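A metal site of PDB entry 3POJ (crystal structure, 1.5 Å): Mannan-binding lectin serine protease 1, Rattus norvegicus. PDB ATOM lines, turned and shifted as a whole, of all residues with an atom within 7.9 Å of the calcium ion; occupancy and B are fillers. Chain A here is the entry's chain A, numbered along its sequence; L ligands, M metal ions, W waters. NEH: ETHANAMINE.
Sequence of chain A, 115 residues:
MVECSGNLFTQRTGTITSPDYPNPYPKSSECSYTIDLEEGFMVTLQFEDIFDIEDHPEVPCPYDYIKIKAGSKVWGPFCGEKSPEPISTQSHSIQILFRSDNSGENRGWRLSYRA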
ATOM      1  N   TYR A  25     -17.238  12.399  -2.557  1.00  0.00           N
ATOM      2  CA  TYR A  25     -18.679  12.159  -2.506  1.00  0.00           C
ATOM      3  C   TYR A  25     -19.366  12.762  -3.747  1.00  0.00           C
ATOM      4  O   TYR A  25     -18.871  13.671  -4.406  1.00  0.00           O
ATOM      5  CB  TYR A  25     -19.314  12.711  -1.243  1.00  0.00           C
ATOM      6  CG  TYR A  25     -18.915  14.138  -0.883  1.00  0.00           C
ATOM      7  CD1 TYR A  25     -19.493  15.254  -1.481  1.00  0.00           C
ATOM      8  CD2 TYR A  25     -17.937  14.398   0.093  1.00  0.00           C
ATOM      9  CE1 TYR A  25     -19.121  16.540  -1.087  1.00  0.00           C
ATOM     10  CE2 TYR A  25     -17.618  15.669   0.531  1.00  0.00           C
ATOM     11  CZ  TYR A  25     -18.197  16.758  -0.078  1.00  0.00           C
ATOM     12  OH  TYR A  25     -17.849  18.010   0.294  1.00  0.00           O
ATOM     13  N   PRO A  26     -20.546  12.219  -4.087  1.00  0.00           N
ATOM     14  CA  PRO A  26     -21.225  12.671  -5.304  1.00  0.00           C
ATOM     15  C   PRO A  26     -21.690  14.110  -5.158  1.00  0.00           C
ATOM     16  O   PRO A  26     -22.090  14.592  -4.082  1.00  0.00           O
ATOM     17  CB  PRO A  26     -22.495  11.749  -5.380  1.00  0.00           C
ATOM     18  CG  PRO A  26     -22.090  10.503  -4.617  1.00  0.00           C
ATOM     19  CD  PRO A  26     -21.216  11.028  -3.505  1.00  0.00           C
ATOM     20  N   LYS A  27     -21.790  14.728  -6.315  1.00  0.00           N
ATOM     21  CA  LYS A  27     -22.479  16.029  -6.383  1.00  0.00           C
ATOM     22  C   LYS A  27     -23.928  15.891  -6.072  1.00  0.00           C
ATOM     23  O   LYS A  27     -24.506  14.854  -6.299  1.00  0.00           O
ATOM     24  CB  LYS A  27     -22.214  16.690  -7.711  1.00  0.00           C
ATOM     25  CG  LYS A  27     -22.900  16.149  -8.733  1.00  0.00           C
ATOM     26  CD  LYS A  27     -22.564  16.872 -10.116  1.00  0.00           C
ATOM     27  CE  LYS A  27     -21.171  16.624 -10.506  1.00  0.00           C
ATOM     28  NZ  LYS A  27     -20.255  17.778 -10.332  1.00  0.00           N
ATOM     29  N   SER A  28     -24.495  16.906  -5.468  1.00  0.00           N
ATOM     30  CA  SER A  28     -25.930  16.995  -5.242  1.00  0.00           C
ATOM     31  C   SER A  28     -26.443  15.872  -4.341  1.00  0.00           C
ATOM     32  O   SER A  28     -27.590  15.379  -4.514  1.00  0.00           O
ATOM     33  CB  SER A  28     -26.655  17.074  -6.570  1.00  0.00           C
ATOM     34  OG  SER A  28     -26.222  18.265  -7.275  1.00  0.00           O
ATOM     35  N   ILE A  53     -14.855  18.252   3.914  1.00  0.00           N
ATOM     36  CA  ILE A  53     -16.074  18.702   3.307  1.00  0.00           C
ATOM     37  C   ILE A  53     -15.786  20.102   2.750  1.00  0.00           C
ATOM     38  O   ILE A  53     -15.133  20.935   3.396  1.00  0.00           O
ATOM     39  CB  ILE A  53     -17.232  18.712   4.312  1.00  0.00           C
ATOM     40  CG1 ILE A  53     -17.534  17.327   4.889  1.00  0.00           C
ATOM     41  CG2 ILE A  53     -18.486  19.351   3.694  1.00  0.00           C
ATOM     42  CD1 ILE A  53     -18.645  17.241   5.936  1.00  0.00           C
ATOM     43  N   GLU A  54     -16.250  20.400   1.534  1.00  0.00           N
ATOM     44  CA  GLU A  54     -15.986  21.739   0.944  1.00  0.00           C
ATOM     45  C   GLU A  54     -16.425  22.827   1.913  1.00  0.00           C
ATOM     46  O   GLU A  54     -17.453  22.707   2.572  1.00  0.00           O
ATOM     47  CB  GLU A  54     -16.803  21.858  -0.306  1.00  0.00           C
ATOM     48  CG  GLU A  54     -16.346  22.977  -1.243  1.00  0.00           C
ATOM     49  CD  GLU A  54     -17.174  23.122  -2.530  1.00  0.00           C
ATOM     50  OE1 GLU A  54     -18.141  22.380  -2.728  1.00  0.00           O
ATOM     51  OE2 GLU A  54     -16.773  24.026  -3.350  1.00  0.00           O
ATOM     52  N   ASP A  55     -15.694  23.907   1.923  1.00  0.00           N
ATOM     53  CA  ASP A  55     -16.002  25.050   2.732  1.00  0.00           C
ATOM     54  C   ASP A  55     -15.841  26.355   1.947  1.00  0.00           C
ATOM     55  O   ASP A  55     -15.676  26.334   0.724  1.00  0.00           O
ATOM     56  CB  ASP A  55     -15.266  25.028   4.076  1.00  0.00           C
ATOM     57  CG  ASP A  55     -13.779  25.277   3.941  1.00  0.00           C
ATOM     58  OD1 ASP A  55     -13.109  25.352   4.998  1.00  0.00           O
ATOM     59  OD2 ASP A  55     -13.280  25.398   2.797  1.00  0.00           O
ATOM     60  N   TYR A  63     -21.966  25.307   1.024  1.00  0.00           N
ATOM     61  CA  TYR A  63     -21.948  24.390  -0.089  1.00  0.00           C
ATOM     62  C   TYR A  63     -22.386  22.990   0.305  1.00  0.00           C
ATOM     63  O   TYR A  63     -23.388  22.486  -0.190  1.00  0.00           O
ATOM     64  CB  TYR A  63     -20.569  24.380  -0.722  1.00  0.00           C
ATOM     65  CG  TYR A  63     -20.123  25.722  -1.267  1.00  0.00           C
ATOM     66  CD1 TYR A  63     -20.960  26.542  -2.000  1.00  0.00           C
ATOM     67  CD2 TYR A  63     -18.827  26.141  -1.067  1.00  0.00           C
ATOM     68  CE1 TYR A  63     -20.512  27.750  -2.506  1.00  0.00           C
ATOM     69  CE2 TYR A  63     -18.370  27.346  -1.597  1.00  0.00           C
ATOM     70  CZ  TYR A  63     -19.222  28.158  -2.334  1.00  0.00           C
ATOM     71  OH  TYR A  63     -18.738  29.334  -2.904  1.00  0.00           O
ATOM     72  N   ASP A  64     -21.566  22.370   1.160  1.00  0.00           N
ATOM     73  CA  ASP A  64     -21.726  21.006   1.580  1.00  0.00           C
ATOM     74  C   ASP A  64     -21.592  20.978   3.093  1.00  0.00           C
ATOM     75  O   ASP A  64     -20.847  21.793   3.686  1.00  0.00           O
ATOM     76  CB  ASP A  64     -20.616  20.139   1.003  1.00  0.00           C
ATOM     77  CG  ASP A  64     -20.345  20.259  -0.508  1.00  0.00           C
ATOM     78  OD1 ASP A  64     -21.144  20.831  -1.274  1.00  0.00           O
ATOM     79  OD2 ASP A  64     -19.268  19.763  -0.926  1.00  0.00           O
ATOM     80  N   TYR A  65     -22.266  20.051   3.771  1.00  0.00           N
ATOM     81  CA  TYR A  65     -22.130  19.946   5.232  1.00  0.00           C
ATOM     82  C   TYR A  65     -22.828  18.736   5.759  1.00  0.00           C
ATOM     83  O   TYR A  65     -23.708  18.165   5.116  1.00  0.00           O
ATOM     84  CB  TYR A  65     -22.698  21.188   5.970  1.00  0.00           C
ATOM     85  CG  TYR A  65     -24.074  21.644   5.591  1.00  0.00           C
ATOM     86  CD1 TYR A  65     -25.198  21.021   6.038  1.00  0.00           C
ATOM     87  CD2 TYR A  65     -24.198  22.722   4.743  1.00  0.00           C
ATOM     88  CE1 TYR A  65     -26.471  21.530   5.672  1.00  0.00           C
ATOM     89  CE2 TYR A  65     -25.486  23.223   4.372  1.00  0.00           C
ATOM     90  CZ  TYR A  65     -26.618  22.593   4.839  1.00  0.00           C
ATOM     91  OH  TYR A  65     -27.825  23.105   4.425  1.00  0.00           O
ATOM     92  N   PHE A  98     -26.544  14.827   5.512  1.00  0.00           N
ATOM     93  CA  PHE A  98     -25.445  15.333   4.713  1.00  0.00           C
ATOM     94  C   PHE A  98     -25.968  15.821   3.407  1.00  0.00           C
ATOM     95  O   PHE A  98     -26.730  15.110   2.717  1.00  0.00           O
ATOM     96  CB  PHE A  98     -24.398  14.193   4.481  1.00  0.00           C
ATOM     97  CG  PHE A  98     -23.303  14.568   3.493  1.00  0.00           C
ATOM     98  CD1 PHE A  98     -22.401  15.522   3.823  1.00  0.00           C
ATOM     99  CD2 PHE A  98     -23.163  13.965   2.275  1.00  0.00           C
ATOM    100  CE1 PHE A  98     -21.384  15.848   2.917  1.00  0.00           C
ATOM    101  CE2 PHE A  98     -22.161  14.279   1.379  1.00  0.00           C
ATOM    102  CZ  PHE A  98     -21.255  15.201   1.704  1.00  0.00           C
ATOM    103  N   ARG A  99     -25.531  17.023   2.996  1.00  0.00           N
ATOM    104  CA  ARG A  99     -25.879  17.560   1.676  1.00  0.00           C
ATOM    105  C   ARG A  99     -24.609  18.041   0.993  1.00  0.00           C
ATOM    106  O   ARG A  99     -23.692  18.547   1.658  1.00  0.00           O
ATOM    107  CB  ARG A  99     -26.917  18.659   1.794  1.00  0.00           C
ATOM    108  CG  ARG A  99     -26.397  19.958   2.401  1.00  0.00           C
ATOM    109  CD  ARG A  99     -26.073  21.042   1.357  1.00  0.00           C
ATOM    110  NE  ARG A  99     -27.279  21.604   0.818  1.00  0.00           N
ATOM    111  CZ  ARG A  99     -27.288  22.557  -0.140  1.00  0.00           C
ATOM    112  NH1 ARG A  99     -28.439  23.044  -0.606  1.00  0.00           N
ATOM    113  NH2 ARG A  99     -26.184  22.987  -0.641  1.00  0.00           N
ATOM    114  N   SER A 100     -24.624  17.941  -0.326  1.00  0.00           N
ATOM    115  CA  SER A 100     -23.590  18.528  -1.129  1.00  0.00           C
ATOM    116  C   SER A 100     -24.183  19.254  -2.315  1.00  0.00           C
ATOM    117  O   SER A 100     -25.247  18.868  -2.799  1.00  0.00           O
ATOM    118  CB  SER A 100     -22.554  17.502  -1.591  1.00  0.00           C
ATOM    119  OG  SER A 100     -23.127  16.571  -2.491  1.00  0.00           O
ATOM    120  N   ASP A 101     -23.453  20.277  -2.784  1.00  0.00           N
ATOM    121  CA  ASP A 101     -23.854  21.036  -3.922  1.00  0.00           C
ATOM    122  C   ASP A 101     -23.325  20.394  -5.212  1.00  0.00           C
ATOM    123  O   ASP A 101     -22.862  19.242  -5.237  1.00  0.00           O
ATOM    124  CB  ASP A 101     -23.432  22.514  -3.722  1.00  0.00           C
ATOM    125  CG  ASP A 101     -21.975  22.772  -3.986  1.00  0.00           C
ATOM    126  OD1 ASP A 101     -21.200  21.760  -4.087  1.00  0.00           O
ATOM    127  OD2 ASP A 101     -21.609  23.970  -3.992  1.00  0.00           O
ATOM    128  N   ASN A 102     -23.395  21.133  -6.327  1.00  0.00           N
ATOM    129  CA  ASN A 102     -23.165  20.476  -7.613  1.00  0.00           C
ATOM    130  C   ASN A 102     -21.747  20.569  -8.133  1.00  0.00           C
ATOM    131  O   ASN A 102     -21.521  20.207  -9.265  1.00  0.00           O
ATOM    132  CB  ASN A 102     -24.128  20.987  -8.688  1.00  0.00           C
ATOM    133  CG  ASN A 102     -24.417  19.958  -9.820  1.00  0.00           C
ATOM    134  OD1 ASN A 102     -24.239  20.299 -11.006  1.00  0.00           O
ATOM    135  ND2 ASN A 102     -24.854  18.725  -9.468  1.00  0.00           N
ATOM    136  N   SER A 103     -20.772  20.906  -7.295  1.00  0.00           N
ATOM    137  CA  SER A 103     -19.414  20.900  -7.745  1.00  0.00           C
ATOM    138  C   SER A 103     -18.432  20.747  -6.626  1.00  0.00           C
ATOM    139  O   SER A 103     -18.778  20.880  -5.440  1.00  0.00           O
ATOM    140  CB  SER A 103     -19.156  22.200  -8.480  1.00  0.00           C
ATOM    141  OG  SER A 103     -19.296  23.381  -7.713  1.00  0.00           O
ATOM    142  N   GLY A 104     -17.178  20.542  -6.994  1.00  0.00           N
ATOM    143  CA  GLY A 104     -16.120  20.384  -6.009  1.00  0.00           C
ATOM    144  C   GLY A 104     -15.604  18.975  -5.911  1.00  0.00           C
ATOM    145  O   GLY A 104     -16.212  18.053  -6.422  1.00  0.00           O
ATOM    146  N   GLU A 105     -14.509  18.804  -5.173  1.00  0.00           N
ATOM    147  CA  GLU A 105     -13.938  17.525  -4.951  1.00  0.00           C
ATOM    148  C   GLU A 105     -13.406  17.469  -3.513  1.00  0.00           C
ATOM    149  O   GLU A 105     -12.435  18.149  -3.187  1.00  0.00           O
ATOM    150  CB  GLU A 105     -12.777  17.308  -5.894  1.00  0.00           C
ATOM    151  CG  GLU A 105     -12.133  15.951  -5.706  1.00  0.00           C
ATOM    152  CD  GLU A 105     -10.909  15.743  -6.602  1.00  0.00           C
ATOM    153  OE1 GLU A 105     -11.163  15.305  -7.790  1.00  0.00           O
ATOM    154  OE2 GLU A 105      -9.726  15.876  -6.073  1.00  0.00           O
ATOM    155  N   ASN A 106     -14.042  16.658  -2.673  1.00  0.00           N
ATOM    156  CA  ASN A 106     -13.700  16.523  -1.279  1.00  0.00           C
ATOM    157  C   ASN A 106     -14.008  15.089  -0.821  1.00  0.00           C
ATOM    158  O   ASN A 106     -14.995  14.496  -1.312  1.00  0.00           O
ATOM    159  CB  ASN A 106     -14.532  17.538  -0.388  1.00  0.00           C
ATOM    160  CG  ASN A 106     -14.248  18.995  -0.709  1.00  0.00           C
ATOM    161  OD1 ASN A 106     -13.236  19.569  -0.148  1.00  0.00           O
ATOM    162  ND2 ASN A 106     -14.966  19.523  -1.647  1.00  0.00           N
HETATM  163  N   NEH L   1     -19.060  24.246  -4.965  1.00  0.00           N
HETATM  164  CA  NEH L   1     -18.975  25.620  -5.074  1.00  0.00           C
HETATM  165  CB  NEH L   1     -19.832  26.243  -5.877  1.00  0.00           C
HETATM  166 CA    CA M   1     -19.368  20.570  -3.211  1.00  0.00          CA
HETATM  167  O   HOH W   1     -17.372  19.106  -3.133  1.00  0.00           O
HETATM  168  O   HOH W   2     -20.453  18.624  -3.968  1.00  0.00           O
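The side-chain carboxylate (OE2) of Glu 54 lies within salt-bridge range of a nitrogen (N) of the ligand (2.8 Å).
O of Ser 103 sits close to N of the ligand (3.4 Å).
N of the ligand sits at hydrogen-bond distance from OG of Ser 103.
The side-chain carboxylate (OD2) of Asp 101 is in salt-bridge range of a nitrogen (N) of the ligand, 2.7 Å away.
The backbone NH (N) of Glu 54 lies within hydrogen-bond range of the side-chain hydroxyl (OH) of Tyr 25, 3.1 Å away.
N of Asp 101 sits at hydrogen-bond distance from O of Tyr 63 (3.4 Å).
The backbone carbonyl oxygen (O) of Asp 101 sits at hydrogen-bond distance from the backbone NH (N) of Ser 28.
OH of Tyr 25 lies close to OD2 of Asp 64 (2.6 Å).
Within 4 Å of the calcium ion: Glu 54, Asp 64, Asp 101 and Ser 103.
The calcium ion is bound by the side-chain carboxylate (OE1) of Glu 54 (2.2 Å), the backbone carbonyl oxygen (O) of Ser 103 (2.3 Å), the side-chain carboxylate (OD1) of Asp 101 (2.4 Å), water W2 (2.4 Å), the side-chain carboxylate (OD2) of Asp 64 (2.4 Å), water W1 (2.5 Å) and the side-chain carboxylate (OD1) of Asp 64 (2.6 Å).
The calcium ion has seven donor atoms within binding distance.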
